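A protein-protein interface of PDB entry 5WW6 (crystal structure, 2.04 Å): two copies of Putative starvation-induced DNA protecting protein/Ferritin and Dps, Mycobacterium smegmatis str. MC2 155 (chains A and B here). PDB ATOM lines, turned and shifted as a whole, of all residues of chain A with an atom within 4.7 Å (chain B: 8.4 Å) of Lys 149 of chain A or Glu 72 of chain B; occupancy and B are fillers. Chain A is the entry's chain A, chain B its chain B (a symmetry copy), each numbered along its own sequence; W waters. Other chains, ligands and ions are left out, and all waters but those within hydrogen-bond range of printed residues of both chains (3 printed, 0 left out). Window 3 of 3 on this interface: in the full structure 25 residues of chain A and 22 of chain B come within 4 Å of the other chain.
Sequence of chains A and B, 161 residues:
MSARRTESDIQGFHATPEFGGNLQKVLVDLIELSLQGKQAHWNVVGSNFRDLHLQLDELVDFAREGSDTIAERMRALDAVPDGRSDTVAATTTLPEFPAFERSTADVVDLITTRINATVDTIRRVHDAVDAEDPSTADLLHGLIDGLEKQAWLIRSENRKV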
ATOM      1  N   ASP A 145     -25.172  20.571  -1.245  1.00  0.00           N
ATOM      2  CA  ASP A 145     -23.884  20.346  -0.575  1.00  0.00           C
ATOM      3  C   ASP A 145     -22.838  19.752  -1.526  1.00  0.00           C
ATOM      4  O   ASP A 145     -21.731  20.283  -1.632  1.00  0.00           O
ATOM      5  CB  ASP A 145     -24.045  19.459   0.676  1.00  0.00           C
ATOM      6  CG  ASP A 145     -24.683  20.200   1.843  1.00  0.00           C
ATOM      7  OD1 ASP A 145     -24.640  21.445   1.840  1.00  0.00           O
ATOM      8  OD2 ASP A 145     -25.239  19.543   2.757  1.00  0.00           O
ATOM      9  N   GLY A 146     -23.191  18.657  -2.199  1.00  0.00           N
ATOM     10  CA  GLY A 146     -22.274  17.954  -3.088  1.00  0.00           C
ATOM     11  C   GLY A 146     -21.874  18.798  -4.289  1.00  0.00           C
ATOM     12  O   GLY A 146     -20.710  18.785  -4.688  1.00  0.00           O
ATOM     13  N   LEU A 147     -22.825  19.542  -4.854  1.00  0.00           N
ATOM     14  CA  LEU A 147     -22.522  20.373  -6.027  1.00  0.00           C
ATOM     15  C   LEU A 147     -21.683  21.602  -5.695  1.00  0.00           C
ATOM     16  O   LEU A 147     -20.763  21.947  -6.442  1.00  0.00           O
ATOM     17  CB  LEU A 147     -23.795  20.783  -6.786  1.00  0.00           C
ATOM     18  CG  LEU A 147     -24.545  19.714  -7.588  1.00  0.00           C
ATOM     19  CD1 LEU A 147     -25.893  20.262  -8.037  1.00  0.00           C
ATOM     20  CD2 LEU A 147     -23.726  19.233  -8.789  1.00  0.00           C
ATOM     21  N   GLU A 148     -22.004  22.265  -4.581  1.00  0.00           N
ATOM     22  CA  GLU A 148     -21.216  23.418  -4.130  1.00  0.00           C
ATOM     23  C   GLU A 148     -19.785  23.022  -3.746  1.00  0.00           C
ATOM     24  O   GLU A 148     -18.867  23.813  -3.920  1.00  0.00           O
ATOM     25  CB  GLU A 148     -21.927  24.186  -3.007  1.00  0.00           C
ATOM     26  CG  GLU A 148     -23.115  24.998  -3.527  1.00  0.00           C
ATOM     27  CD  GLU A 148     -23.972  25.636  -2.440  1.00  0.00           C
ATOM     28  OE1 GLU A 148     -23.933  25.204  -1.274  1.00  0.00           O
ATOM     29  OE2 GLU A 148     -24.712  26.582  -2.764  1.00  0.00           O
ATOM     30  N   LYS A 149     -19.603  21.802  -3.245  1.00  0.00           N
ATOM     31  CA  LYS A 149     -18.258  21.243  -3.047  1.00  0.00           C
ATOM     32  C   LYS A 149     -17.527  21.075  -4.391  1.00  0.00           C
ATOM     33  O   LYS A 149     -16.368  21.467  -4.508  1.00  0.00           O
ATOM     34  CB  LYS A 149     -18.304  19.930  -2.263  1.00  0.00           C
ATOM     35  CG  LYS A 149     -16.927  19.373  -1.908  1.00  0.00           C
ATOM     36  CD  LYS A 149     -17.017  18.025  -1.202  1.00  0.00           C
ATOM     37  CE  LYS A 149     -15.660  17.331  -1.246  1.00  0.00           C
ATOM     38  NZ  LYS A 149     -15.562  16.238  -0.236  1.00  0.00           N
ATOM     39  N   GLN A 150     -18.210  20.515  -5.396  1.00  0.00           N
ATOM     40  CA  GLN A 150     -17.643  20.400  -6.755  1.00  0.00           C
ATOM     41  C   GLN A 150     -17.222  21.767  -7.312  1.00  0.00           C
ATOM     42  O   GLN A 150     -16.114  21.907  -7.826  1.00  0.00           O
ATOM     43  CB  GLN A 150     -18.613  19.685  -7.717  1.00  0.00           C
ATOM     44  CG  GLN A 150     -18.777  18.176  -7.481  1.00  0.00           C
ATOM     45  CD  GLN A 150     -17.463  17.400  -7.570  1.00  0.00           C
ATOM     46  OE1 GLN A 150     -16.757  17.454  -8.585  1.00  0.00           O
ATOM     47  NE2 GLN A 150     -17.138  16.664  -6.504  1.00  0.00           N
ATOM     48  N   ALA A 151     -18.099  22.766  -7.159  1.00  0.00           N
ATOM     49  CA  ALA A 151     -17.838  24.140  -7.603  1.00  0.00           C
ATOM     50  C   ALA A 151     -16.572  24.686  -6.947  1.00  0.00           C
ATOM     51  O   ALA A 151     -15.730  25.242  -7.636  1.00  0.00           O
ATOM     52  CB  ALA A 151     -19.031  25.050  -7.323  1.00  0.00           C
ATOM     53  N   TRP A 152     -16.430  24.492  -5.631  1.00  0.00           N
ATOM     54  CA  TRP A 152     -15.209  24.881  -4.921  1.00  0.00           C
ATOM     55  C   TRP A 152     -13.952  24.193  -5.475  1.00  0.00           C
ATOM     56  O   TRP A 152     -12.960  24.872  -5.764  1.00  0.00           O
ATOM     57  CB  TRP A 152     -15.344  24.649  -3.411  1.00  0.00           C
ATOM     58  CG  TRP A 152     -14.028  24.649  -2.656  1.00  0.00           C
ATOM     59  CD1 TRP A 152     -13.090  25.653  -2.609  1.00  0.00           C
ATOM     60  CD2 TRP A 152     -13.528  23.593  -1.834  1.00  0.00           C
ATOM     61  NE1 TRP A 152     -12.033  25.274  -1.810  1.00  0.00           N
ATOM     62  CE2 TRP A 152     -12.281  24.017  -1.318  1.00  0.00           C
ATOM     63  CE3 TRP A 152     -14.024  22.326  -1.467  1.00  0.00           C
ATOM     64  CZ2 TRP A 152     -11.512  23.218  -0.457  1.00  0.00           C
ATOM     65  CZ3 TRP A 152     -13.257  21.531  -0.617  1.00  0.00           C
ATOM     66  CH2 TRP A 152     -12.014  21.982  -0.119  1.00  0.00           C
ATOM     67  N   LEU A 153     -14.011  22.865  -5.629  1.00  0.00           N
ATOM     68  CA  LEU A 153     -12.865  22.078  -6.094  1.00  0.00           C
ATOM     69  C   LEU A 153     -12.434  22.421  -7.517  1.00  0.00           C
ATOM     70  O   LEU A 153     -11.247  22.338  -7.838  1.00  0.00           O
ATOM     71  CB  LEU A 153     -13.133  20.575  -5.961  1.00  0.00           C
ATOM     72  CG  LEU A 153     -13.329  20.010  -4.544  1.00  0.00           C
ATOM     73  CD1 LEU A 153     -13.932  18.608  -4.626  1.00  0.00           C
ATOM     74  CD2 LEU A 153     -12.025  20.003  -3.741  1.00  0.00           C
ATOM     75  N   LEU B  23     -19.688  28.465  11.789  1.00  0.00           N
ATOM     76  CA  LEU B  23     -19.076  27.197  11.407  1.00  0.00           C
ATOM     77  C   LEU B  23     -17.671  27.072  11.977  1.00  0.00           C
ATOM     78  O   LEU B  23     -17.262  25.986  12.372  1.00  0.00           O
ATOM     79  CB  LEU B  23     -19.092  26.998   9.881  1.00  0.00           C
ATOM     80  CG  LEU B  23     -20.453  26.811   9.185  1.00  0.00           C
ATOM     81  CD1 LEU B  23     -20.260  26.302   7.758  1.00  0.00           C
ATOM     82  CD2 LEU B  23     -21.390  25.887   9.956  1.00  0.00           C
ATOM     83  N   LEU B  27     -15.953  24.065  14.033  1.00  0.00           N
ATOM     84  CA  LEU B  27     -14.676  23.516  13.585  1.00  0.00           C
ATOM     85  C   LEU B  27     -13.639  23.358  14.702  1.00  0.00           C
ATOM     86  O   LEU B  27     -13.075  22.276  14.853  1.00  0.00           O
ATOM     87  CB  LEU B  27     -14.098  24.330  12.417  1.00  0.00           C
ATOM     88  CG  LEU B  27     -12.728  23.877  11.877  1.00  0.00           C
ATOM     89  CD1 LEU B  27     -12.814  22.546  11.135  1.00  0.00           C
ATOM     90  CD2 LEU B  27     -12.108  24.947  10.993  1.00  0.00           C
ATOM     91  N   GLU B  65     -13.429  13.393  10.438  1.00  0.00           N
ATOM     92  CA  GLU B  65     -14.282  13.467   9.243  1.00  0.00           C
ATOM     93  C   GLU B  65     -15.182  14.691   9.351  1.00  0.00           C
ATOM     94  O   GLU B  65     -15.385  15.402   8.377  1.00  0.00           O
ATOM     95  CB  GLU B  65     -15.146  12.207   9.078  1.00  0.00           C
ATOM     96  CG  GLU B  65     -14.378  10.960   8.679  1.00  0.00           C
ATOM     97  N   GLY B  66     -15.711  14.918  10.554  1.00  0.00           N
ATOM     98  CA  GLY B  66     -16.573  16.056  10.847  1.00  0.00           C
ATOM     99  C   GLY B  66     -15.904  17.396  10.615  1.00  0.00           C
ATOM    100  O   GLY B  66     -16.493  18.272   9.983  1.00  0.00           O
ATOM    101  N   SER B  67     -14.678  17.557  11.123  1.00  0.00           N
ATOM    102  CA  SER B  67     -13.950  18.817  10.959  1.00  0.00           C
ATOM    103  C   SER B  67     -13.641  19.081   9.486  1.00  0.00           C
ATOM    104  O   SER B  67     -13.747  20.223   9.029  1.00  0.00           O
ATOM    105  CB  SER B  67     -12.702  18.894  11.860  1.00  0.00           C
ATOM    106  OG  SER B  67     -11.817  17.838  11.598  1.00  0.00           O
ATOM    107  N   ASP B  68     -13.317  18.015   8.745  1.00  0.00           N
ATOM    108  CA  ASP B  68     -13.126  18.130   7.306  1.00  0.00           C
ATOM    109  C   ASP B  68     -14.423  18.581   6.622  1.00  0.00           C
ATOM    110  O   ASP B  68     -14.393  19.529   5.847  1.00  0.00           O
ATOM    111  CB  ASP B  68     -12.575  16.832   6.696  1.00  0.00           C
ATOM    112  CG  ASP B  68     -11.980  17.044   5.306  1.00  0.00           C
ATOM    113  OD1 ASP B  68     -12.508  16.435   4.354  1.00  0.00           O
ATOM    114  OD2 ASP B  68     -11.008  17.830   5.155  1.00  0.00           O
ATOM    115  N   THR B  69     -15.543  17.935   6.956  1.00  0.00           N
ATOM    116  CA  THR B  69     -16.864  18.277   6.418  1.00  0.00           C
ATOM    117  C   THR B  69     -17.199  19.765   6.645  1.00  0.00           C
ATOM    118  O   THR B  69     -17.606  20.454   5.712  1.00  0.00           O
ATOM    119  CB  THR B  69     -17.944  17.352   7.019  1.00  0.00           C
ATOM    120  OG1 THR B  69     -17.632  15.997   6.672  1.00  0.00           O
ATOM    121  CG2 THR B  69     -19.354  17.706   6.506  1.00  0.00           C
ATOM    122  N   ILE B  70     -16.967  20.252   7.862  1.00  0.00           N
ATOM    123  CA  ILE B  70     -17.283  21.646   8.219  1.00  0.00           C
ATOM    124  C   ILE B  70     -16.359  22.644   7.506  1.00  0.00           C
ATOM    125  O   ILE B  70     -16.821  23.647   6.958  1.00  0.00           O
ATOM    126  CB  ILE B  70     -17.273  21.851   9.759  1.00  0.00           C
ATOM    127  CG1 ILE B  70     -18.428  21.055  10.413  1.00  0.00           C
ATOM    128  CG2 ILE B  70     -17.286  23.342  10.153  1.00  0.00           C
ATOM    129  CD1 ILE B  70     -19.846  21.518  10.079  1.00  0.00           C
ATOM    130  N   ALA B  71     -15.061  22.359   7.526  1.00  0.00           N
ATOM    131  CA  ALA B  71     -14.068  23.222   6.888  1.00  0.00           C
ATOM    132  C   ALA B  71     -14.296  23.308   5.384  1.00  0.00           C
ATOM    133  O   ALA B  71     -14.192  24.384   4.801  1.00  0.00           O
ATOM    134  CB  ALA B  71     -12.664  22.734   7.195  1.00  0.00           C
ATOM    135  N   GLU B  72     -14.644  22.181   4.774  1.00  0.00           N
ATOM    136  CA  GLU B  72     -14.889  22.147   3.336  1.00  0.00           C
ATOM    137  C   GLU B  72     -16.217  22.798   2.966  1.00  0.00           C
ATOM    138  O   GLU B  72     -16.317  23.405   1.910  1.00  0.00           O
ATOM    139  CB  GLU B  72     -14.773  20.724   2.790  1.00  0.00           C
ATOM    140  CG  GLU B  72     -13.344  20.215   2.927  1.00  0.00           C
ATOM    141  CD  GLU B  72     -13.036  18.980   2.117  1.00  0.00           C
ATOM    142  OE1 GLU B  72     -11.830  18.783   1.843  1.00  0.00           O
ATOM    143  OE2 GLU B  72     -13.961  18.215   1.772  1.00  0.00           O
ATOM    144  N   ARG B  73     -17.214  22.695   3.845  1.00  0.00           N
ATOM    145  CA  ARG B  73     -18.474  23.422   3.651  1.00  0.00           C
ATOM    146  C   ARG B  73     -18.246  24.941   3.709  1.00  0.00           C
ATOM    147  O   ARG B  73     -18.817  25.691   2.909  1.00  0.00           O
ATOM    148  CB  ARG B  73     -19.550  22.966   4.661  1.00  0.00           C
ATOM    149  CG  ARG B  73     -20.933  23.596   4.457  1.00  0.00           C
ATOM    150  CD  ARG B  73     -21.485  23.312   3.068  1.00  0.00           C
ATOM    151  NE  ARG B  73     -22.796  23.917   2.807  1.00  0.00           N
ATOM    152  CZ  ARG B  73     -23.274  24.165   1.586  1.00  0.00           C
ATOM    153  NH1 ARG B  73     -22.556  23.871   0.492  1.00  0.00           N
ATOM    154  NH2 ARG B  73     -24.474  24.714   1.451  1.00  0.00           N
ATOM    155  N   MET B  74     -17.405  25.378   4.645  1.00  0.00           N
ATOM    156  CA  MET B  74     -16.972  26.775   4.728  1.00  0.00           C
ATOM    157  C   MET B  74     -16.352  27.210   3.405  1.00  0.00           C
ATOM    158  O   MET B  74     -16.769  28.209   2.817  1.00  0.00           O
ATOM    159  CB  MET B  74     -15.977  26.988   5.880  1.00  0.00           C
ATOM    160  CG  MET B  74     -16.583  26.793   7.263  1.00  0.00           C
ATOM    161  SD  MET B  74     -15.412  26.914   8.626  1.00  0.00           S
ATOM    162  CE  MET B  74     -15.084  28.682   8.651  1.00  0.00           C
ATOM    163  N   ARG B  75     -15.386  26.431   2.923  1.00  0.00           N
ATOM    164  CA  ARG B  75     -14.730  26.727   1.643  1.00  0.00           C
ATOM    165  C   ARG B  75     -15.706  26.744   0.461  1.00  0.00           C
ATOM    166  O   ARG B  75     -15.619  27.623  -0.405  1.00  0.00           O
ATOM    167  CB  ARG B  75     -13.564  25.758   1.393  1.00  0.00           C
ATOM    168  CG  ARG B  75     -12.392  25.902   2.364  1.00  0.00           C
ATOM    169  CD  ARG B  75     -11.746  27.285   2.330  1.00  0.00           C
ATOM    170  NE  ARG B  75     -11.164  27.604   1.033  1.00  0.00           N
ATOM    171  CZ  ARG B  75     -11.543  28.608   0.249  1.00  0.00           C
ATOM    172  NH1 ARG B  75     -12.501  29.458   0.622  1.00  0.00           N
ATOM    173  NH2 ARG B  75     -10.934  28.778  -0.915  1.00  0.00           N
ATOM    174  N   ALA B  76     -16.641  25.790   0.443  1.00  0.00           N
ATOM    175  CA  ALA B  76     -17.669  25.724  -0.599  1.00  0.00           C
ATOM    176  C   ALA B  76     -18.462  27.035  -0.660  1.00  0.00           C
ATOM    177  O   ALA B  76     -18.784  27.529  -1.741  1.00  0.00           O
ATOM    178  CB  ALA B  76     -18.603  24.547  -0.358  1.00  0.00           C
ATOM    179  N   LEU B  77     -18.730  27.612   0.511  1.00  0.00           N
ATOM    180  CA  LEU B  77     -19.475  28.859   0.589  1.00  0.00           C
ATOM    181  C   LEU B  77     -18.569  30.098   0.661  1.00  0.00           C
ATOM    182  O   LEU B  77     -19.031  31.197   0.958  1.00  0.00           O
ATOM    183  CB  LEU B  77     -20.488  28.795   1.746  1.00  0.00           C
ATOM    184  CG  LEU B  77     -21.609  27.739   1.614  1.00  0.00           C
ATOM    185  CD1 LEU B  77     -22.603  27.850   2.753  1.00  0.00           C
ATOM    186  CD2 LEU B  77     -22.359  27.817   0.286  1.00  0.00           C
ATOM    187  N   ASP B  78     -17.288  29.896   0.356  1.00  0.00           N
ATOM    188  CA  ASP B  78     -16.254  30.942   0.364  1.00  0.00           C
ATOM    189  C   ASP B  78     -15.956  31.589   1.719  1.00  0.00           C
ATOM    190  O   ASP B  78     -15.438  32.700   1.780  1.00  0.00           O
ATOM    191  CB  ASP B  78     -16.452  31.980  -0.772  1.00  0.00           C
ATOM    192  CG  ASP B  78     -15.411  31.848  -1.881  1.00  0.00           C
ATOM    193  OD1 ASP B  78     -14.372  31.170  -1.678  1.00  0.00           O
ATOM    194  OD2 ASP B  78     -15.605  32.452  -2.955  1.00  0.00           O
ATOM    195  N   ALA B  79     -16.268  30.874   2.807  1.00  0.00           N
ATOM    196  CA  ALA B  79     -15.698  31.185   4.113  1.00  0.00           C
ATOM    197  C   ALA B  79     -14.294  30.552   4.166  1.00  0.00           C
ATOM    198  O   ALA B  79     -13.924  29.749   3.285  1.00  0.00           O
ATOM    199  CB  ALA B  79     -16.593  30.669   5.236  1.00  0.00           C
ATOM    200  N   PRO B  81     -11.682  28.619   6.806  1.00  0.00           N
ATOM    201  CA  PRO B  81     -11.506  27.984   8.114  1.00  0.00           C
ATOM    202  C   PRO B  81     -10.151  28.289   8.735  1.00  0.00           C
ATOM    203  O   PRO B  81      -9.196  28.605   8.015  1.00  0.00           O
ATOM    204  CB  PRO B  81     -11.590  26.493   7.785  1.00  0.00           C
ATOM    205  CG  PRO B  81     -11.137  26.395   6.368  1.00  0.00           C
ATOM    206  CD  PRO B  81     -11.739  27.614   5.731  1.00  0.00           C
ATOM    207  N   LEU B 139     -25.849  18.944   7.684  1.00  0.00           N
ATOM    208  CA  LEU B 139     -24.510  18.468   8.084  1.00  0.00           C
ATOM    209  C   LEU B 139     -24.343  18.540   9.601  1.00  0.00           C
ATOM    210  O   LEU B 139     -23.789  17.630  10.222  1.00  0.00           O
ATOM    211  CB  LEU B 139     -23.383  19.254   7.373  1.00  0.00           C
ATOM    212  CG  LEU B 139     -23.393  19.257   5.834  1.00  0.00           C
ATOM    213  CD1 LEU B 139     -22.326  20.191   5.278  1.00  0.00           C
ATOM    214  CD2 LEU B 139     -23.234  17.844   5.265  1.00  0.00           C
HETATM  215  O   HOH W   1      -9.256  26.321  -1.145  1.00  0.00           O
HETATM  216  O   HOH W   2     -16.292  17.427   2.528  1.00  0.00           O
HETATM  217  O   HOH W   3     -20.421  21.817   0.246  1.00  0.00           O
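The side-chain carboxylate (OD1) of Asp 145 of chain A is in salt-bridge range of the guanidinium group (NE) of Arg 73 of chain B.
NH1 of Arg 73 of chain B lies within salt-bridge range of OE1 of Glu 148 of chain A (2.6 Å).
The side-chain carboxylate (OE2) of Glu 72 of chain B is in salt-bridge range of the side-chain amino group (NZ) of Lys 149 of chain A (3.2 Å).
NH1 of Arg 75 of chain B is in salt-bridge range of OD1 of Asp 78 of chain B (3.4 Å).
O of Ala 79 of chain B is in hydrogen-bond range of NH1 of Arg 75 of chain B, at 3.0 Å.
Asp 145 of chain A touches Leu 139 of chain B.
Ala 76 of chain B touches Glu 148 of chain A.
CD2 of Leu 77 of chain B touches OE1 of Glu 148 of chain A, 3.4 Å away.
Trp 152 of chain A touches Glu 72 of chain B (CZ3 to CD, 3.7 Å).
Arg 75 of chain B touches Trp 152 of chain A.
Trp 152 of chain A touches Ala 76 of chain B (CB to CA, 3.8 Å).
Of chain B, only Glu 72 comes within 4 Å of Lys 149 of chain A.
Glu 72 of chain B touches just these residues of chain A: Lys 149 (3.2 Å) and Trp 152 (3.7 Å).
Of the printed residues of chain A, Arg 73 of chain B touches Asp 145 and Glu 148.
Of the printed residues of chain B, Asp 145 of chain A touches Arg 73 and Leu 139.
Printed residues of chain B within 4 Å of Trp 152 of chain A: Glu 72, Arg 75 and Ala 76.
Leu 23 of chain B touches none of the printed residues of chain A.
The nearest residue of chain B that does not touch Lys 149 of chain A is Ala 76 of chain B (4.1 Å).
Hydrophobic or aromatic side chains of chain B that line the printed part of chain A: Ala 76, Leu 77 and Leu 139.
Hydrophobic or aromatic side chains of chain A within 4 Å of the printed part of chain B: Trp 152.
Along chain A the printed residues that touch a printed residue of chain B span positions 145 to 152.
No position is printed for both chains.
Of the 9 pairs that touch across the chains among the printed residues, none has its exchanged pair printed and touching as well.
Water W2 bridges the side-chain carboxylate (OE2) of Glu 72 of chain B (2.6 Å) and the side-chain amino group (NZ) of Lys 149 of chain A (3.1 Å).
Water W3 bridges O of Asp 145 of chain A and NH1 of Arg 73 of chain B.
Water W1 lies within hydrogen-bond range of the guanidinium group of Arg 75 of chain B (3.0 Å) and the indole nitrogen of Trp 152 of chain A (3.0 Å).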
